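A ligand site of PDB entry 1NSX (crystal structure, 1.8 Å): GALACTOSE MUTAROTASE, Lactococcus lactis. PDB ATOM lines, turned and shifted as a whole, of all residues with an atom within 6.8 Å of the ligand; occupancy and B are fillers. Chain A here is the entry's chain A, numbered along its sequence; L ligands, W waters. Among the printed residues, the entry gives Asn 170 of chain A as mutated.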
ATOM      1  N   ASP A  58     -14.200   3.204  11.605  1.00  0.00           N
ATOM      2  CA  ASP A  58     -14.903   4.287  10.966  1.00  0.00           C
ATOM      3  C   ASP A  58     -14.068   5.508  11.250  1.00  0.00           C
ATOM      4  O   ASP A  58     -13.914   5.864  12.407  1.00  0.00           O
ATOM      5  CB  ASP A  58     -16.313   4.481  11.550  1.00  0.00           C
ATOM      6  CG  ASP A  58     -17.041   5.629  10.893  1.00  0.00           C
ATOM      7  OD1 ASP A  58     -16.584   6.318  10.007  1.00  0.00           O
ATOM      8  OD2 ASP A  58     -18.262   5.765  11.337  1.00  0.00           O
ATOM      9  N   TYR A  60     -14.598   8.581  10.449  1.00  0.00           N
ATOM     10  CA  TYR A  60     -15.214   9.893  10.515  1.00  0.00           C
ATOM     11  C   TYR A  60     -15.551  10.474  11.863  1.00  0.00           C
ATOM     12  O   TYR A  60     -15.479  11.711  12.040  1.00  0.00           O
ATOM     13  CB  TYR A  60     -16.511   9.921   9.696  1.00  0.00           C
ATOM     14  CG  TYR A  60     -16.250   9.920   8.196  1.00  0.00           C
ATOM     15  CD1 TYR A  60     -16.830   8.930   7.392  1.00  0.00           C
ATOM     16  CD2 TYR A  60     -15.483  10.901   7.582  1.00  0.00           C
ATOM     17  CE1 TYR A  60     -16.636   8.899   6.011  1.00  0.00           C
ATOM     18  CE2 TYR A  60     -15.276  10.885   6.211  1.00  0.00           C
ATOM     19  CZ  TYR A  60     -15.851   9.887   5.434  1.00  0.00           C
ATOM     20  OH  TYR A  60     -15.663   9.872   4.075  1.00  0.00           O
ATOM     21  N   PRO A  61     -15.962   9.649  12.805  1.00  0.00           N
ATOM     22  CA  PRO A  61     -16.362  10.208  14.097  1.00  0.00           C
ATOM     23  C   PRO A  61     -15.394  11.176  14.760  1.00  0.00           C
ATOM     24  O   PRO A  61     -14.255  10.826  14.994  1.00  0.00           O
ATOM     25  CB  PRO A  61     -16.708   9.024  15.005  1.00  0.00           C
ATOM     26  CG  PRO A  61     -16.912   7.872  14.044  1.00  0.00           C
ATOM     27  CD  PRO A  61     -16.144   8.184  12.763  1.00  0.00           C
ATOM     28  N   VAL A  65     -13.616  17.233   8.718  1.00  0.00           N
ATOM     29  CA  VAL A  65     -13.872  16.701   7.376  1.00  0.00           C
ATOM     30  C   VAL A  65     -13.852  17.849   6.390  1.00  0.00           C
ATOM     31  O   VAL A  65     -14.282  18.953   6.709  1.00  0.00           O
ATOM     32  CB  VAL A  65     -15.149  15.872   7.146  1.00  0.00           C
ATOM     33  CG1 VAL A  65     -15.078  14.570   7.964  1.00  0.00           C
ATOM     34  CG2 VAL A  65     -16.315  16.681   7.663  1.00  0.00           C
ATOM     35  N   ALA A  69     -17.407  19.588   3.218  1.00  0.00           N
ATOM     36  CA  ALA A  69     -18.135  18.584   3.984  1.00  0.00           C
ATOM     37  C   ALA A  69     -19.449  18.205   3.285  1.00  0.00           C
ATOM     38  O   ALA A  69     -20.156  19.050   2.693  1.00  0.00           O
ATOM     39  CB  ALA A  69     -18.371  19.133   5.389  1.00  0.00           C
ATOM     40  N   GLY A  70     -19.813  16.928   3.336  1.00  0.00           N
ATOM     41  CA  GLY A  70     -21.034  16.522   2.691  1.00  0.00           C
ATOM     42  C   GLY A  70     -20.831  15.924   1.329  1.00  0.00           C
ATOM     43  O   GLY A  70     -19.685  15.683   0.941  1.00  0.00           O
ATOM     44  N   ARG A  71     -21.957  15.717   0.619  1.00  0.00           N
ATOM     45  CA  ARG A  71     -21.936  15.148  -0.722  1.00  0.00           C
ATOM     46  C   ARG A  71     -22.079  16.166  -1.817  1.00  0.00           C
ATOM     47  O   ARG A  71     -22.994  17.009  -1.804  1.00  0.00           O
ATOM     48  CB  ARG A  71     -23.138  14.251  -0.963  1.00  0.00           C
ATOM     49  CG  ARG A  71     -23.004  13.059  -0.066  1.00  0.00           C
ATOM     50  CD  ARG A  71     -24.270  12.182  -0.070  1.00  0.00           C
ATOM     51  NE  ARG A  71     -23.969  11.006   0.780  1.00  0.00           N
ATOM     52  CZ  ARG A  71     -24.182  10.932   2.098  1.00  0.00           C
ATOM     53  NH1 ARG A  71     -24.787  11.905   2.823  1.00  0.00           N
ATOM     54  NH2 ARG A  71     -23.786   9.833   2.685  1.00  0.00           N
ATOM     55  N   GLU A  90     -18.109   7.800  -3.257  1.00  0.00           N
ATOM     56  CA  GLU A  90     -19.352   7.191  -2.780  1.00  0.00           C
ATOM     57  C   GLU A  90     -20.143   7.121  -4.046  1.00  0.00           C
ATOM     58  O   GLU A  90     -20.900   8.046  -4.362  1.00  0.00           O
ATOM     59  CB  GLU A  90     -20.095   8.170  -1.891  1.00  0.00           C
ATOM     60  CG  GLU A  90     -21.141   7.346  -1.144  1.00  0.00           C
ATOM     61  CD  GLU A  90     -22.090   8.181  -0.321  1.00  0.00           C
ATOM     62  OE1 GLU A  90     -22.633   9.160  -0.780  1.00  0.00           O
ATOM     63  OE2 GLU A  90     -22.349   7.715   0.876  1.00  0.00           O
ATOM     64  N   LEU A  95     -17.913  12.548  -1.258  1.00  0.00           N
ATOM     65  CA  LEU A  95     -18.432  12.691   0.090  1.00  0.00           C
ATOM     66  C   LEU A  95     -17.297  13.075   1.023  1.00  0.00           C
ATOM     67  O   LEU A  95     -16.265  12.440   1.042  1.00  0.00           O
ATOM     68  CB  LEU A  95     -18.975  11.321   0.562  1.00  0.00           C
ATOM     69  CG  LEU A  95     -19.208  11.276   2.086  1.00  0.00           C
ATOM     70  CD1 LEU A  95     -20.395  12.138   2.550  1.00  0.00           C
ATOM     71  CD2 LEU A  95     -19.462   9.848   2.480  1.00  0.00           C
ATOM     72  N   HIS A  96     -17.489  14.099   1.812  1.00  0.00           N
ATOM     73  CA  HIS A  96     -16.434  14.493   2.743  1.00  0.00           C
ATOM     74  C   HIS A  96     -15.007  14.669   2.163  1.00  0.00           C
ATOM     75  O   HIS A  96     -14.000  14.295   2.763  1.00  0.00           O
ATOM     76  CB  HIS A  96     -16.381  13.534   3.932  1.00  0.00           C
ATOM     77  CG  HIS A  96     -17.647  13.638   4.736  1.00  0.00           C
ATOM     78  ND1 HIS A  96     -18.423  14.783   4.702  1.00  0.00           N
ATOM     79  CD2 HIS A  96     -18.203  12.740   5.577  1.00  0.00           C
ATOM     80  CE1 HIS A  96     -19.432  14.574   5.514  1.00  0.00           C
ATOM     81  NE2 HIS A  96     -19.342  13.359   6.060  1.00  0.00           N
ATOM     82  N   THR A 168     -16.198  20.853   8.211  1.00  0.00           N
ATOM     83  CA  THR A 168     -17.065  20.733   9.398  1.00  0.00           C
ATOM     84  C   THR A 168     -16.422  19.792  10.400  1.00  0.00           C
ATOM     85  O   THR A 168     -15.432  19.105  10.088  1.00  0.00           O
ATOM     86  CB  THR A 168     -18.547  20.390   9.110  1.00  0.00           C
ATOM     87  OG1 THR A 168     -19.341  20.798  10.230  1.00  0.00           O
ATOM     88  CG2 THR A 168     -18.748  18.888   8.814  1.00  0.00           C
ATOM     89  N   ASN A 170     -17.126  16.584  12.810  1.00  0.00           N
ATOM     90  CA  ASN A 170     -18.039  15.454  12.859  1.00  0.00           C
ATOM     91  C   ASN A 170     -18.232  14.693  14.197  1.00  0.00           C
ATOM     92  O   ASN A 170     -18.343  13.459  14.221  1.00  0.00           O
ATOM     93  CB  ASN A 170     -17.678  14.497  11.710  1.00  0.00           C
ATOM     94  CG  ASN A 170     -18.898  13.801  11.132  1.00  0.00           C
ATOM     95  OD1 ASN A 170     -18.869  12.628  10.801  1.00  0.00           O
ATOM     96  ND2 ASN A 170     -19.996  14.536  11.086  1.00  0.00           N
ATOM     97  N   TYR A 172     -20.116  13.030  17.258  1.00  0.00           N
ATOM     98  CA  TYR A 172     -21.407  12.393  17.475  1.00  0.00           C
ATOM     99  C   TYR A 172     -21.655  12.464  18.982  1.00  0.00           C
ATOM    100  O   TYR A 172     -20.835  12.000  19.784  1.00  0.00           O
ATOM    101  CB  TYR A 172     -21.379  10.870  17.235  1.00  0.00           C
ATOM    102  CG  TYR A 172     -21.420  10.491  15.776  1.00  0.00           C
ATOM    103  CD1 TYR A 172     -20.258  10.455  15.012  1.00  0.00           C
ATOM    104  CD2 TYR A 172     -22.621  10.168  15.156  1.00  0.00           C
ATOM    105  CE1 TYR A 172     -20.297  10.085  13.663  1.00  0.00           C
ATOM    106  CE2 TYR A 172     -22.695   9.806  13.810  1.00  0.00           C
ATOM    107  CZ  TYR A 172     -21.519   9.771  13.066  1.00  0.00           C
ATOM    108  OH  TYR A 172     -21.570   9.390  11.731  1.00  0.00           O
ATOM    109  N   GLU A 203     -28.712  10.166  -1.430  1.00  0.00           N
ATOM    110  CA  GLU A 203     -28.565  11.270  -0.512  1.00  0.00           C
ATOM    111  C   GLU A 203     -28.104  12.551  -1.119  1.00  0.00           C
ATOM    112  O   GLU A 203     -27.632  13.413  -0.413  1.00  0.00           O
ATOM    113  CB  GLU A 203     -27.889  10.915   0.798  1.00  0.00           C
ATOM    114  CG  GLU A 203     -28.630   9.773   1.572  1.00  0.00           C
ATOM    115  CD  GLU A 203     -27.813   8.807   2.442  1.00  0.00           C
ATOM    116  OE1 GLU A 203     -27.361   7.700   2.147  1.00  0.00           O
ATOM    117  OE2 GLU A 203     -27.774   9.214   3.666  1.00  0.00           O
ATOM    118  N   ASP A 243     -30.901  12.767   8.417  1.00  0.00           N
ATOM    119  CA  ASP A 243     -29.619  12.879   7.702  1.00  0.00           C
ATOM    120  C   ASP A 243     -29.772  14.082   6.783  1.00  0.00           C
ATOM    121  O   ASP A 243     -29.700  13.965   5.575  1.00  0.00           O
ATOM    122  CB  ASP A 243     -29.232  11.611   6.928  1.00  0.00           C
ATOM    123  CG  ASP A 243     -27.777  11.645   6.584  1.00  0.00           C
ATOM    124  OD1 ASP A 243     -27.083  12.589   6.870  1.00  0.00           O
ATOM    125  OD2 ASP A 243     -27.336  10.563   6.001  1.00  0.00           O
ATOM    126  N   HIS A 244     -30.030  15.252   7.386  1.00  0.00           N
ATOM    127  CA  HIS A 244     -30.347  16.428   6.586  1.00  0.00           C
ATOM    128  C   HIS A 244     -29.867  17.743   7.136  1.00  0.00           C
ATOM    129  O   HIS A 244     -29.742  17.943   8.337  1.00  0.00           O
ATOM    130  CB  HIS A 244     -31.890  16.618   6.753  1.00  0.00           C
ATOM    131  CG  HIS A 244     -32.714  15.532   6.116  1.00  0.00           C
ATOM    132  ND1 HIS A 244     -32.958  14.282   6.732  1.00  0.00           N
ATOM    133  CD2 HIS A 244     -33.337  15.533   4.906  1.00  0.00           C
ATOM    134  CE1 HIS A 244     -33.669  13.535   5.906  1.00  0.00           C
ATOM    135  NE2 HIS A 244     -33.916  14.277   4.813  1.00  0.00           N
ATOM    136  N   VAL A 277     -26.084  20.220   9.719  1.00  0.00           N
ATOM    137  CA  VAL A 277     -26.520  18.952   9.191  1.00  0.00           C
ATOM    138  C   VAL A 277     -26.710  17.978  10.345  1.00  0.00           C
ATOM    139  O   VAL A 277     -25.782  17.754  11.155  1.00  0.00           O
ATOM    140  CB  VAL A 277     -25.465  18.388   8.272  1.00  0.00           C
ATOM    141  CG1 VAL A 277     -25.943  16.991   7.853  1.00  0.00           C
ATOM    142  CG2 VAL A 277     -25.467  19.347   7.079  1.00  0.00           C
ATOM    143  N   ILE A 278     -27.896  17.390  10.457  1.00  0.00           N
ATOM    144  CA  ILE A 278     -28.147  16.458  11.555  1.00  0.00           C
ATOM    145  C   ILE A 278     -28.226  15.027  11.096  1.00  0.00           C
ATOM    146  O   ILE A 278     -29.059  14.715  10.244  1.00  0.00           O
ATOM    147  CB  ILE A 278     -29.405  16.877  12.338  1.00  0.00           C
ATOM    148  CG1 ILE A 278     -29.086  18.211  12.993  1.00  0.00           C
ATOM    149  CG2 ILE A 278     -29.848  15.857  13.387  1.00  0.00           C
ATOM    150  CD1 ILE A 278     -30.263  18.781  13.742  1.00  0.00           C
ATOM    151  N   PHE A 279     -27.340  14.183  11.610  1.00  0.00           N
ATOM    152  CA  PHE A 279     -27.356  12.774  11.206  1.00  0.00           C
ATOM    153  C   PHE A 279     -27.457  11.942  12.460  1.00  0.00           C
ATOM    154  O   PHE A 279     -26.639  12.116  13.389  1.00  0.00           O
ATOM    155  CB  PHE A 279     -26.062  12.457  10.413  1.00  0.00           C
ATOM    156  CG  PHE A 279     -25.772  10.997  10.144  1.00  0.00           C
ATOM    157  CD1 PHE A 279     -26.663  10.240   9.394  1.00  0.00           C
ATOM    158  CD2 PHE A 279     -24.600  10.400  10.636  1.00  0.00           C
ATOM    159  CE1 PHE A 279     -26.435   8.897   9.104  1.00  0.00           C
ATOM    160  CE2 PHE A 279     -24.358   9.058  10.367  1.00  0.00           C
ATOM    161  CZ  PHE A 279     -25.259   8.333   9.591  1.00  0.00           C
ATOM    162  N   PHE A 283     -27.308   3.560  11.242  1.00  0.00           N
ATOM    163  CA  PHE A 283     -26.536   2.396  10.771  1.00  0.00           C
ATOM    164  C   PHE A 283     -27.168   1.008  10.804  1.00  0.00           C
ATOM    165  O   PHE A 283     -26.482  -0.015  10.610  1.00  0.00           O
ATOM    166  CB  PHE A 283     -25.145   2.328  11.394  1.00  0.00           C
ATOM    167  CG  PHE A 283     -24.359   3.614  11.252  1.00  0.00           C
ATOM    168  CD1 PHE A 283     -23.989   4.393  12.357  1.00  0.00           C
ATOM    169  CD2 PHE A 283     -23.949   4.030   9.988  1.00  0.00           C
ATOM    170  CE1 PHE A 283     -23.214   5.546  12.201  1.00  0.00           C
ATOM    171  CE2 PHE A 283     -23.196   5.200   9.797  1.00  0.00           C
ATOM    172  CZ  PHE A 283     -22.840   5.944  10.924  1.00  0.00           C
ATOM    173  N   THR A 302     -25.207  13.941  15.179  1.00  0.00           N
ATOM    174  CA  THR A 302     -24.249  14.994  14.886  1.00  0.00           C
ATOM    175  C   THR A 302     -24.871  16.352  14.801  1.00  0.00           C
ATOM    176  O   THR A 302     -26.055  16.448  14.633  1.00  0.00           O
ATOM    177  CB  THR A 302     -23.649  14.817  13.477  1.00  0.00           C
ATOM    178  OG1 THR A 302     -24.678  15.018  12.506  1.00  0.00           O
ATOM    179  CG2 THR A 302     -23.028  13.438  13.309  1.00  0.00           C
ATOM    180  N   GLU A 304     -23.379  19.006  12.447  1.00  0.00           N
ATOM    181  CA  GLU A 304     -22.316  19.480  11.565  1.00  0.00           C
ATOM    182  C   GLU A 304     -22.639  20.895  11.081  1.00  0.00           C
ATOM    183  O   GLU A 304     -23.462  21.085  10.190  1.00  0.00           O
ATOM    184  CB  GLU A 304     -22.177  18.530  10.361  1.00  0.00           C
ATOM    185  CG  GLU A 304     -21.797  17.094  10.794  1.00  0.00           C
ATOM    186  CD  GLU A 304     -22.087  16.107   9.673  1.00  0.00           C
ATOM    187  OE1 GLU A 304     -22.419  16.463   8.578  1.00  0.00           O
ATOM    188  OE2 GLU A 304     -22.025  14.852   9.981  1.00  0.00           O
ATOM    189  N   GLN A 306     -22.119  24.104   8.996  1.00  0.00           N
ATOM    190  CA  GLN A 306     -21.392  24.443   7.765  1.00  0.00           C
ATOM    191  C   GLN A 306     -22.388  25.080   6.818  1.00  0.00           C
ATOM    192  O   GLN A 306     -23.549  25.310   7.183  1.00  0.00           O
ATOM    193  CB  GLN A 306     -20.904  23.133   7.084  1.00  0.00           C
ATOM    194  CG  GLN A 306     -22.122  22.181   6.896  1.00  0.00           C
ATOM    195  CD  GLN A 306     -21.809  20.881   6.143  1.00  0.00           C
ATOM    196  OE1 GLN A 306     -21.594  19.823   6.778  1.00  0.00           O
ATOM    197  NE2 GLN A 306     -21.753  20.934   4.808  1.00  0.00           N
ATOM    198  N   PRO A 309     -24.903  21.355   2.304  1.00  0.00           N
ATOM    199  CA  PRO A 309     -24.494  20.662   1.093  1.00  0.00           C
ATOM    200  C   PRO A 309     -25.568  20.920   0.006  1.00  0.00           C
ATOM    201  O   PRO A 309     -26.692  21.268   0.305  1.00  0.00           O
ATOM    202  CB  PRO A 309     -24.582  19.151   1.413  1.00  0.00           C
ATOM    203  CG  PRO A 309     -24.756  19.062   2.930  1.00  0.00           C
ATOM    204  CD  PRO A 309     -25.079  20.451   3.465  1.00  0.00           C
HETATM  205  C1  LIG L   1     -22.905  12.728   7.447  1.00  0.00           C
HETATM  206  C2  LIG L   1     -23.635  12.149   6.217  1.00  0.00           C
HETATM  207  C3  LIG L   1     -24.124  10.775   6.591  1.00  0.00           C
HETATM  208  C4  LIG L   1     -22.904   9.901   6.859  1.00  0.00           C
HETATM  209  C5  LIG L   1     -22.054  10.531   7.958  1.00  0.00           C
HETATM  210  C6  LIG L   1     -20.724   9.837   8.142  1.00  0.00           C
HETATM  211  O1  LIG L   1     -22.398  14.013   7.107  1.00  0.00           O
HETATM  212  O2  LIG L   1     -24.748  12.941   5.743  1.00  0.00           O
HETATM  213  O3  LIG L   1     -24.877  10.172   5.534  1.00  0.00           O
HETATM  214  O4  LIG L   1     -22.108   9.732   5.693  1.00  0.00           O
HETATM  215  O5  LIG L   1     -21.738  11.906   7.654  1.00  0.00           O
HETATM  216  O6  LIG L   1     -20.019  10.727   8.997  1.00  0.00           O
HETATM  217  O   HOH W   1     -25.170   7.468   5.707  1.00  0.00           O
HETATM  218  O   HOH W   2     -24.052  15.517   4.698  1.00  0.00           O
HETATM  219  O   HOH W   3     -22.266  17.218   6.181  1.00  0.00           O
HETATM  220  O   HOH W   4     -19.490   8.073  10.691  1.00  0.00           O
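Residues that only touch the ligand: Glu 203, Phe 279 and Tyr 60. Hydrophobic or aromatic side chains within 4 Å of the ligand: Tyr 60, His 96 and Phe 279. Along chain A the residues within 4 Å of the ligand span positions 60 to 304. The nearest printed residue that does not touch the ligand is Leu 95 (4.2 Å).
OD2 of Asp 243 lies close to OE2 of Glu 203. N of Asp 243 sits close to O of Ile 278, at 3.2 Å. N of Val 277 is in hydrogen-bond range of O of Glu 304, 2.8 Å away. NE of Arg 71 is in salt-bridge range of OE1 of Glu 90 (2.8 Å). The backbone carbonyl oxygen (O) of Gly 70 lies within hydrogen-bond range of the backbone NH (N) of His 96 (2.8 Å). The backbone NH (N) of Thr 302 is in hydrogen-bond range of the backbone carbonyl oxygen (O) of Phe 279 (2.9 Å). OD1 of Asp 58 lies within hydrogen-bond range of N of Tyr 60, 3.0 Å away.
Water W4 lies within hydrogen-bond range of the side-chain hydroxyl (OH) of Tyr 172 (2.7 Å), the side-chain carboxylate (OD2) of Asp 58 (2.7 Å) and an oxygen (O6) of the ligand (3.2 Å). Water W3 lies within hydrogen-bond range of OE1 of Glu 304, OE1 of Gln 306 and O1 of the ligand.
The side-chain carboxylate (OD2) of Asp 243 is in hydrogen-bond range of an oxygen (O3) of the ligand, at 2.5 Å. OE1 of Glu 304 is in hydrogen-bond range of O1 of the ligand (2.9 Å). The side-chain amide oxygen (OD1) of Asn 170 sits at hydrogen-bond distance from an oxygen (O6) of the ligand. O3 of the ligand sits at hydrogen-bond distance from NH2 of Arg 71 (3.1 Å). A ring nitrogen (NE2) of His 96 lies within hydrogen-bond range of an oxygen (O5) of the ligand, at 3.2 Å. The side-chain hydroxyl (OH) of Tyr 172 lies within hydrogen-bond range of an oxygen (O6) of the ligand (3.4 Å).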
